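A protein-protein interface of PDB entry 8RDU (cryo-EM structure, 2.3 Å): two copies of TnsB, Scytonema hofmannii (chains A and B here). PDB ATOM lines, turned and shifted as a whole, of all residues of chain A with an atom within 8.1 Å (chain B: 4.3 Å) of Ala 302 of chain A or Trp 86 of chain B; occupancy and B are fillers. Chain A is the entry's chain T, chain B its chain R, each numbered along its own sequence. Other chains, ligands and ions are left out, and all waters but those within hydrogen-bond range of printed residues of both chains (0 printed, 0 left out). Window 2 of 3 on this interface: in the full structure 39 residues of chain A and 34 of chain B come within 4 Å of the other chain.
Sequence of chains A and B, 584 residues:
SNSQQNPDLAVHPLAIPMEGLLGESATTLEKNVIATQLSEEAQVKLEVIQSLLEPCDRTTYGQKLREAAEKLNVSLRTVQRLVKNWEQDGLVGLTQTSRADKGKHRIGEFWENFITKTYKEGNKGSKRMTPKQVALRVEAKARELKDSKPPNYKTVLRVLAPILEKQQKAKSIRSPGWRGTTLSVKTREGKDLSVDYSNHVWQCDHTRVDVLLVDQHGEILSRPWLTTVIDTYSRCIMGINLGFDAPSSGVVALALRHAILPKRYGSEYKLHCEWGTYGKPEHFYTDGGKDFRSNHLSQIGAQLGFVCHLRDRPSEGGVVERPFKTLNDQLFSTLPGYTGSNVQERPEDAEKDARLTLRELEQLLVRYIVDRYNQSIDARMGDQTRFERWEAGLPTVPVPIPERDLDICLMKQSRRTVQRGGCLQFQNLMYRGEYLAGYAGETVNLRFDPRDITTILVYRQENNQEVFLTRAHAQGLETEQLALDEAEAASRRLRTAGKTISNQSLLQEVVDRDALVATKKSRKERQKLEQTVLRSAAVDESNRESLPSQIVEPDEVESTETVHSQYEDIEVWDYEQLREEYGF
The backbone NH (N) of Leu 91 of chain B lies within hydrogen-bond range of the side-chain amide oxygen (OE1) of Gln 303 of chain A, at 3.1 Å.
O of His 296 of chain A sits close to OE1 of Gln 299 of chain A. The indole nitrogen (NE1) of Trp 86 of chain B sits at hydrogen-bond distance from the side-chain carboxylate (OE2) of Glu 87 of chain B.
Among the printed residues, pairs that only touch across the chains: Gln 299 of chain A with Leu 91 of chain B (3.9 Å), Ala 302 of chain A with Leu 46 of chain B (3.7 Å), Ala 302 of chain A with Trp 86 of chain B (2.8 Å), Gln 303 of chain A with Trp 86 of chain B (3.5 Å) and Gln 303 of chain A with Gly 90 of chain B (3.5 Å).
Ala 302 of chain A touches just these residues of chain B: Leu 46 (3.7 Å) and Trp 86 (2.8 Å). Trp 86 of chain B touches two residues of chain A. Of chain A, only Gln 303 comes within 4 Å of Gly 90 of chain B. Of the printed residues of chain A, Leu 91 of chain B touches Gln 299 (3.9 Å) and Gln 303 (3.1 Å). Of the printed residues of chain B, Gln 303 of chain A touches Trp 86, Gly 90 and Leu 91. Of the printed residues of chain B, Gln 299 of chain A touches Leu 91 (3.9 Å). Of the printed residues of chain A, Leu 46 of chain B touches Ala 302. Asp 89 of chain B touches none of the printed residues of chain A. Lys 84 of chain B touches none of the printed residues of chain A. The nearest printed residue of chain B that does not touch Ala 302 of chain A is Leu 91 of chain B (4.5 Å). The nearest residue of chain A that does not touch Trp 86 of chain B is Gly 305 of chain A (4.8 Å).
Printed residues of chain B that touch a printed residue of chain A: Leu 46, Trp 86, Gly 90 and Leu 91. Hydrophobic or aromatic side chains of chain B that line the printed part of chain A: Leu 46, Trp 86 and Leu 91. Hydrophobic or aromatic side chains of chain A that line the printed part of chain B: Ala 302. Among the printed residues, 6 pairs touch across the chains. Among the printed residues, no Asp or Glu carboxylate lies within 4 Å of a Lys or Arg side-chain nitrogen of the other chain.
No position is printed for both chains. Of the 6 pairs that touch across the chains among the printed residues, none has its exchanged pair printed and touching as well.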
ATOM      1  N   LYS A 280      15.043   8.023  18.126  1.00  0.00           N
ATOM      2  CA  LYS A 280      14.859   9.446  17.874  1.00  0.00           C
ATOM      3  C   LYS A 280      13.486   9.723  17.270  1.00  0.00           C
ATOM      4  O   LYS A 280      13.181   9.206  16.188  1.00  0.00           O
ATOM      5  CB  LYS A 280      15.989   9.928  16.966  1.00  0.00           C
ATOM      6  CG  LYS A 280      15.956  11.385  16.533  1.00  0.00           C
ATOM      7  CD  LYS A 280      15.735  11.540  15.048  1.00  0.00           C
ATOM      8  CE  LYS A 280      15.567  13.005  14.689  1.00  0.00           C
ATOM      9  NZ  LYS A 280      16.861  13.734  14.771  1.00  0.00           N
ATOM     10  N   HIS A 296      11.657  27.013  25.089  1.00  0.00           N
ATOM     11  CA  HIS A 296      12.814  26.115  25.148  1.00  0.00           C
ATOM     12  C   HIS A 296      12.604  24.792  24.424  1.00  0.00           C
ATOM     13  O   HIS A 296      13.566  24.207  23.916  1.00  0.00           O
ATOM     14  CB  HIS A 296      13.186  25.818  26.600  1.00  0.00           C
ATOM     15  CG  HIS A 296      14.384  24.927  26.738  1.00  0.00           C
ATOM     16  ND1 HIS A 296      15.642  25.295  26.313  1.00  0.00           N
ATOM     17  CD2 HIS A 296      14.506  23.672  27.230  1.00  0.00           C
ATOM     18  CE1 HIS A 296      16.489  24.308  26.548  1.00  0.00           C
ATOM     19  NE2 HIS A 296      15.825  23.313  27.107  1.00  0.00           N
ATOM     20  N   LEU A 297      11.367  24.303  24.370  1.00  0.00           N
ATOM     21  CA  LEU A 297      11.076  23.097  23.607  1.00  0.00           C
ATOM     22  C   LEU A 297      11.528  23.214  22.157  1.00  0.00           C
ATOM     23  O   LEU A 297      11.961  22.225  21.556  1.00  0.00           O
ATOM     24  CB  LEU A 297       9.577  22.804  23.679  1.00  0.00           C
ATOM     25  CG  LEU A 297       8.999  22.524  25.071  1.00  0.00           C
ATOM     26  CD1 LEU A 297       8.470  23.799  25.712  1.00  0.00           C
ATOM     27  CD2 LEU A 297       7.911  21.466  25.015  1.00  0.00           C
ATOM     28  N   SER A 298      11.457  24.419  21.592  1.00  0.00           N
ATOM     29  CA  SER A 298      11.882  24.656  20.214  1.00  0.00           C
ATOM     30  C   SER A 298      13.378  24.437  20.020  1.00  0.00           C
ATOM     31  O   SER A 298      13.797  23.821  19.033  1.00  0.00           O
ATOM     32  CB  SER A 298      11.497  26.071  19.789  1.00  0.00           C
ATOM     33  OG  SER A 298      11.843  26.310  18.438  1.00  0.00           O
ATOM     34  N   GLN A 299      14.199  24.939  20.942  1.00  0.00           N
ATOM     35  CA  GLN A 299      15.638  24.714  20.861  1.00  0.00           C
ATOM     36  C   GLN A 299      15.997  23.234  20.930  1.00  0.00           C
ATOM     37  O   GLN A 299      16.873  22.768  20.194  1.00  0.00           O
ATOM     38  CB  GLN A 299      16.334  25.473  21.988  1.00  0.00           C
ATOM     39  CG  GLN A 299      16.330  26.976  21.823  1.00  0.00           C
ATOM     40  CD  GLN A 299      15.067  27.605  22.373  1.00  0.00           C
ATOM     41  OE1 GLN A 299      14.022  26.962  22.438  1.00  0.00           O
ATOM     42  NE2 GLN A 299      15.159  28.866  22.780  1.00  0.00           N
ATOM     43  N   ILE A 300      15.333  22.474  21.801  1.00  0.00           N
ATOM     44  CA  ILE A 300      15.577  21.035  21.854  1.00  0.00           C
ATOM     45  C   ILE A 300      15.185  20.381  20.539  1.00  0.00           C
ATOM     46  O   ILE A 300      15.971  19.643  19.933  1.00  0.00           O
ATOM     47  CB  ILE A 300      14.829  20.398  23.034  1.00  0.00           C
ATOM     48  CG1 ILE A 300      15.393  20.900  24.362  1.00  0.00           C
ATOM     49  CG2 ILE A 300      14.941  18.891  22.955  1.00  0.00           C
ATOM     50  CD1 ILE A 300      14.586  20.464  25.558  1.00  0.00           C
ATOM     51  N   GLY A 301      13.959  20.639  20.083  1.00  0.00           N
ATOM     52  CA  GLY A 301      13.508  20.077  18.821  1.00  0.00           C
ATOM     53  C   GLY A 301      14.456  20.375  17.680  1.00  0.00           C
ATOM     54  O   GLY A 301      14.803  19.492  16.893  1.00  0.00           O
ATOM     55  N   ALA A 302      14.904  21.627  17.589  1.00  0.00           N
ATOM     56  CA  ALA A 302      15.895  22.005  16.587  1.00  0.00           C
ATOM     57  C   ALA A 302      17.183  21.207  16.742  1.00  0.00           C
ATOM     58  O   ALA A 302      17.595  20.496  15.823  1.00  0.00           O
ATOM     59  CB  ALA A 302      16.179  23.505  16.677  1.00  0.00           C
ATOM     60  N   GLN A 303      17.790  21.251  17.930  1.00  0.00           N
ATOM     61  CA  GLN A 303      19.086  20.606  18.127  1.00  0.00           C
ATOM     62  C   GLN A 303      19.015  19.105  17.889  1.00  0.00           C
ATOM     63  O   GLN A 303      19.973  18.506  17.385  1.00  0.00           O
ATOM     64  CB  GLN A 303      19.607  20.909  19.533  1.00  0.00           C
ATOM     65  CG  GLN A 303      20.943  20.257  19.882  1.00  0.00           C
ATOM     66  CD  GLN A 303      22.101  20.735  19.026  1.00  0.00           C
ATOM     67  OE1 GLN A 303      21.958  21.632  18.198  1.00  0.00           O
ATOM     68  NE2 GLN A 303      23.265  20.138  19.236  1.00  0.00           N
ATOM     69  N   LEU A 304      17.899  18.475  18.238  1.00  0.00           N
ATOM     70  CA  LEU A 304      17.737  17.052  17.977  1.00  0.00           C
ATOM     71  C   LEU A 304      17.215  16.776  16.574  1.00  0.00           C
ATOM     72  O   LEU A 304      17.138  15.610  16.175  1.00  0.00           O
ATOM     73  CB  LEU A 304      16.799  16.418  19.008  1.00  0.00           C
ATOM     74  CG  LEU A 304      17.220  16.621  20.461  1.00  0.00           C
ATOM     75  CD1 LEU A 304      16.376  15.772  21.384  1.00  0.00           C
ATOM     76  CD2 LEU A 304      18.687  16.298  20.626  1.00  0.00           C
ATOM     77  N   GLY A 305      16.871  17.817  15.824  1.00  0.00           N
ATOM     78  CA  GLY A 305      16.417  17.675  14.457  1.00  0.00           C
ATOM     79  C   GLY A 305      15.067  17.015  14.300  1.00  0.00           C
ATOM     80  O   GLY A 305      14.902  16.135  13.452  1.00  0.00           O
ATOM     81  N   PHE A 306      14.092  17.417  15.112  1.00  0.00           N
ATOM     82  CA  PHE A 306      12.714  17.001  14.904  1.00  0.00           C
ATOM     83  C   PHE A 306      11.799  18.204  15.084  1.00  0.00           C
ATOM     84  O   PHE A 306      12.039  19.052  15.946  1.00  0.00           O
ATOM     85  CB  PHE A 306      12.321  15.845  15.841  1.00  0.00           C
ATOM     86  CG  PHE A 306      12.323  16.193  17.305  1.00  0.00           C
ATOM     87  CD1 PHE A 306      11.294  16.934  17.869  1.00  0.00           C
ATOM     88  CD2 PHE A 306      13.347  15.755  18.123  1.00  0.00           C
ATOM     89  CE1 PHE A 306      11.293  17.241  19.210  1.00  0.00           C
ATOM     90  CE2 PHE A 306      13.350  16.057  19.467  1.00  0.00           C
ATOM     91  CZ  PHE A 306      12.320  16.803  20.010  1.00  0.00           C
ATOM     92  N   VAL A 307      10.760  18.282  14.254  1.00  0.00           N
ATOM     93  CA  VAL A 307       9.849  19.416  14.307  1.00  0.00           C
ATOM     94  C   VAL A 307       9.066  19.379  15.609  1.00  0.00           C
ATOM     95  O   VAL A 307       8.471  18.354  15.966  1.00  0.00           O
ATOM     96  CB  VAL A 307       8.905  19.412  13.095  1.00  0.00           C
ATOM     97  CG1 VAL A 307       7.870  20.516  13.223  1.00  0.00           C
ATOM     98  CG2 VAL A 307       9.689  19.577  11.801  1.00  0.00           C
ATOM     99  N   CYS A 308       9.074  20.490  16.333  1.00  0.00           N
ATOM    100  CA  CYS A 308       8.158  20.687  17.445  1.00  0.00           C
ATOM    101  C   CYS A 308       7.075  21.659  16.998  1.00  0.00           C
ATOM    102  O   CYS A 308       7.374  22.792  16.607  1.00  0.00           O
ATOM    103  CB  CYS A 308       8.893  21.216  18.676  1.00  0.00           C
ATOM    104  SG  CYS A 308       7.887  21.301  20.174  1.00  0.00           S
ATOM    105  N   ILE A 408      20.972  18.603  26.918  1.00  0.00           N
ATOM    106  CA  ILE A 408      20.143  19.801  26.863  1.00  0.00           C
ATOM    107  C   ILE A 408      18.797  19.545  27.514  1.00  0.00           C
ATOM    108  O   ILE A 408      18.192  20.453  28.093  1.00  0.00           O
ATOM    109  CB  ILE A 408      19.989  20.266  25.403  1.00  0.00           C
ATOM    110  CG1 ILE A 408      21.360  20.579  24.803  1.00  0.00           C
ATOM    111  CG2 ILE A 408      19.075  21.472  25.309  1.00  0.00           C
ATOM    112  CD1 ILE A 408      21.303  21.360  23.511  1.00  0.00           C
ATOM    113  N   LEU B  46      17.859  30.555  14.058  1.00  0.00           N
ATOM    114  CA  LEU B  46      17.020  29.470  14.559  1.00  0.00           C
ATOM    115  C   LEU B  46      15.642  29.464  13.906  1.00  0.00           C
ATOM    116  O   LEU B  46      15.137  28.405  13.512  1.00  0.00           O
ATOM    117  CB  LEU B  46      16.881  29.588  16.074  1.00  0.00           C
ATOM    118  CG  LEU B  46      15.889  28.642  16.741  1.00  0.00           C
ATOM    119  CD1 LEU B  46      16.328  27.204  16.556  1.00  0.00           C
ATOM    120  CD2 LEU B  46      15.748  28.985  18.212  1.00  0.00           C
ATOM    121  N   ILE B  49      15.939  27.887  10.632  1.00  0.00           N
ATOM    122  CA  ILE B  49      16.266  26.470  10.790  1.00  0.00           C
ATOM    123  C   ILE B  49      15.045  25.672  11.242  1.00  0.00           C
ATOM    124  O   ILE B  49      14.781  24.576  10.733  1.00  0.00           O
ATOM    125  CB  ILE B  49      17.458  26.298  11.751  1.00  0.00           C
ATOM    126  CG1 ILE B  49      18.765  26.717  11.067  1.00  0.00           C
ATOM    127  CG2 ILE B  49      17.558  24.868  12.247  1.00  0.00           C
ATOM    128  CD1 ILE B  49      19.173  25.828   9.919  1.00  0.00           C
ATOM    129  N   LEU B  82      24.895  28.132   6.130  1.00  0.00           N
ATOM    130  CA  LEU B  82      24.213  28.082   7.422  1.00  0.00           C
ATOM    131  C   LEU B  82      23.726  26.676   7.769  1.00  0.00           C
ATOM    132  O   LEU B  82      24.029  26.153   8.848  1.00  0.00           O
ATOM    133  CB  LEU B  82      23.050  29.074   7.430  1.00  0.00           C
ATOM    134  CG  LEU B  82      22.070  28.958   8.595  1.00  0.00           C
ATOM    135  CD1 LEU B  82      22.782  29.253   9.894  1.00  0.00           C
ATOM    136  CD2 LEU B  82      20.894  29.902   8.410  1.00  0.00           C
ATOM    137  N   VAL B  83      22.968  26.045   6.872  1.00  0.00           N
ATOM    138  CA  VAL B  83      22.511  24.677   7.116  1.00  0.00           C
ATOM    139  C   VAL B  83      23.686  23.704   7.167  1.00  0.00           C
ATOM    140  O   VAL B  83      23.667  22.732   7.931  1.00  0.00           O
ATOM    141  CB  VAL B  83      21.459  24.257   6.069  1.00  0.00           C
ATOM    142  CG1 VAL B  83      20.250  25.177   6.140  1.00  0.00           C
ATOM    143  CG2 VAL B  83      22.043  24.225   4.669  1.00  0.00           C
ATOM    144  N   LYS B  84      24.720  23.941   6.360  1.00  0.00           N
ATOM    145  CA  LYS B  84      25.939  23.144   6.457  1.00  0.00           C
ATOM    146  C   LYS B  84      26.510  23.188   7.869  1.00  0.00           C
ATOM    147  O   LYS B  84      26.707  22.150   8.510  1.00  0.00           O
ATOM    148  CB  LYS B  84      26.969  23.672   5.454  1.00  0.00           C
ATOM    149  CG  LYS B  84      28.325  22.989   5.493  1.00  0.00           C
ATOM    150  CD  LYS B  84      29.295  23.686   4.546  1.00  0.00           C
ATOM    151  CE  LYS B  84      29.043  23.349   3.089  1.00  0.00           C
ATOM    152  NZ  LYS B  84      29.615  22.032   2.708  1.00  0.00           N
ATOM    153  N   ASN B  85      26.774  24.393   8.372  1.00  0.00           N
ATOM    154  CA  ASN B  85      27.329  24.554   9.712  1.00  0.00           C
ATOM    155  C   ASN B  85      26.361  24.080  10.788  1.00  0.00           C
ATOM    156  O   ASN B  85      26.784  23.543  11.817  1.00  0.00           O
ATOM    157  CB  ASN B  85      27.727  26.008   9.953  1.00  0.00           C
ATOM    158  CG  ASN B  85      29.014  26.385   9.246  1.00  0.00           C
ATOM    159  OD1 ASN B  85      29.513  25.641   8.405  1.00  0.00           O
ATOM    160  ND2 ASN B  85      29.564  27.544   9.592  1.00  0.00           N
ATOM    161  N   TRP B  86      25.060  24.284  10.578  1.00  0.00           N
ATOM    162  CA  TRP B  86      24.072  23.727  11.496  1.00  0.00           C
ATOM    163  C   TRP B  86      24.194  22.215  11.624  1.00  0.00           C
ATOM    164  O   TRP B  86      24.157  21.675  12.733  1.00  0.00           O
ATOM    165  CB  TRP B  86      22.661  24.090  11.045  1.00  0.00           C
ATOM    166  CG  TRP B  86      21.726  23.003  11.379  1.00  0.00           C
ATOM    167  CD1 TRP B  86      21.220  22.055  10.541  1.00  0.00           C
ATOM    168  CD2 TRP B  86      21.261  22.677  12.681  1.00  0.00           C
ATOM    169  NE1 TRP B  86      20.422  21.186  11.240  1.00  0.00           N
ATOM    170  CE2 TRP B  86      20.438  21.546  12.561  1.00  0.00           C
ATOM    171  CE3 TRP B  86      21.447  23.247  13.941  1.00  0.00           C
ATOM    172  CZ2 TRP B  86      19.799  20.981  13.652  1.00  0.00           C
ATOM    173  CZ3 TRP B  86      20.817  22.685  15.016  1.00  0.00           C
ATOM    174  CH2 TRP B  86      20.007  21.564  14.869  1.00  0.00           C
ATOM    175  N   GLU B  87      24.311  21.506  10.508  1.00  0.00           N
ATOM    176  CA  GLU B  87      24.516  20.065  10.608  1.00  0.00           C
ATOM    177  C   GLU B  87      25.900  19.752  11.155  1.00  0.00           C
ATOM    178  O   GLU B  87      26.070  18.804  11.930  1.00  0.00           O
ATOM    179  CB  GLU B  87      24.294  19.395   9.255  1.00  0.00           C
ATOM    180  CG  GLU B  87      22.835  19.350   8.850  1.00  0.00           C
ATOM    181  CD  GLU B  87      21.996  18.521   9.804  1.00  0.00           C
ATOM    182  OE1 GLU B  87      22.527  17.546  10.374  1.00  0.00           O
ATOM    183  OE2 GLU B  87      20.807  18.851   9.990  1.00  0.00           O
ATOM    184  N   GLN B  88      26.896  20.552  10.776  1.00  0.00           N
ATOM    185  CA  GLN B  88      28.271  20.288  11.174  1.00  0.00           C
ATOM    186  C   GLN B  88      28.462  20.446  12.678  1.00  0.00           C
ATOM    187  O   GLN B  88      29.252  19.713  13.283  1.00  0.00           O
ATOM    188  CB  GLN B  88      29.209  21.222  10.410  1.00  0.00           C
ATOM    189  CG  GLN B  88      30.670  20.812  10.411  1.00  0.00           C
ATOM    190  CD  GLN B  88      30.960  19.670   9.453  1.00  0.00           C
ATOM    191  OE1 GLN B  88      30.049  19.074   8.876  1.00  0.00           O
ATOM    192  NE2 GLN B  88      32.240  19.369   9.266  1.00  0.00           N
ATOM    193  N   ASP B  89      27.769  21.404  13.300  1.00  0.00           N
ATOM    194  CA  ASP B  89      28.020  21.706  14.708  1.00  0.00           C
ATOM    195  C   ASP B  89      26.775  21.947  15.553  1.00  0.00           C
ATOM    196  O   ASP B  89      26.908  22.072  16.772  1.00  0.00           O
ATOM    197  CB  ASP B  89      28.940  22.927  14.821  1.00  0.00           C
ATOM    198  CG  ASP B  89      30.342  22.644  14.315  1.00  0.00           C
ATOM    199  OD1 ASP B  89      31.059  21.845  14.954  1.00  0.00           O
ATOM    200  OD2 ASP B  89      30.726  23.217  13.273  1.00  0.00           O
ATOM    201  N   GLY B  90      25.583  21.978  14.973  1.00  0.00           N
ATOM    202  CA  GLY B  90      24.374  22.262  15.725  1.00  0.00           C
ATOM    203  C   GLY B  90      24.130  23.747  15.955  1.00  0.00           C
ATOM    204  O   GLY B  90      24.558  24.601  15.179  1.00  0.00           O
ATOM    205  N   LEU B  91      23.424  24.047  17.048  1.00  0.00           N
ATOM    206  CA  LEU B  91      23.131  25.435  17.392  1.00  0.00           C
ATOM    207  C   LEU B  91      24.386  26.271  17.618  1.00  0.00           C
ATOM    208  O   LEU B  91      24.362  27.486  17.400  1.00  0.00           O
ATOM    209  CB  LEU B  91      22.248  25.477  18.636  1.00  0.00           C
ATOM    210  CG  LEU B  91      20.862  24.868  18.468  1.00  0.00           C
ATOM    211  CD1 LEU B  91      20.071  24.982  19.752  1.00  0.00           C
ATOM    212  CD2 LEU B  91      20.140  25.552  17.338  1.00  0.00           C
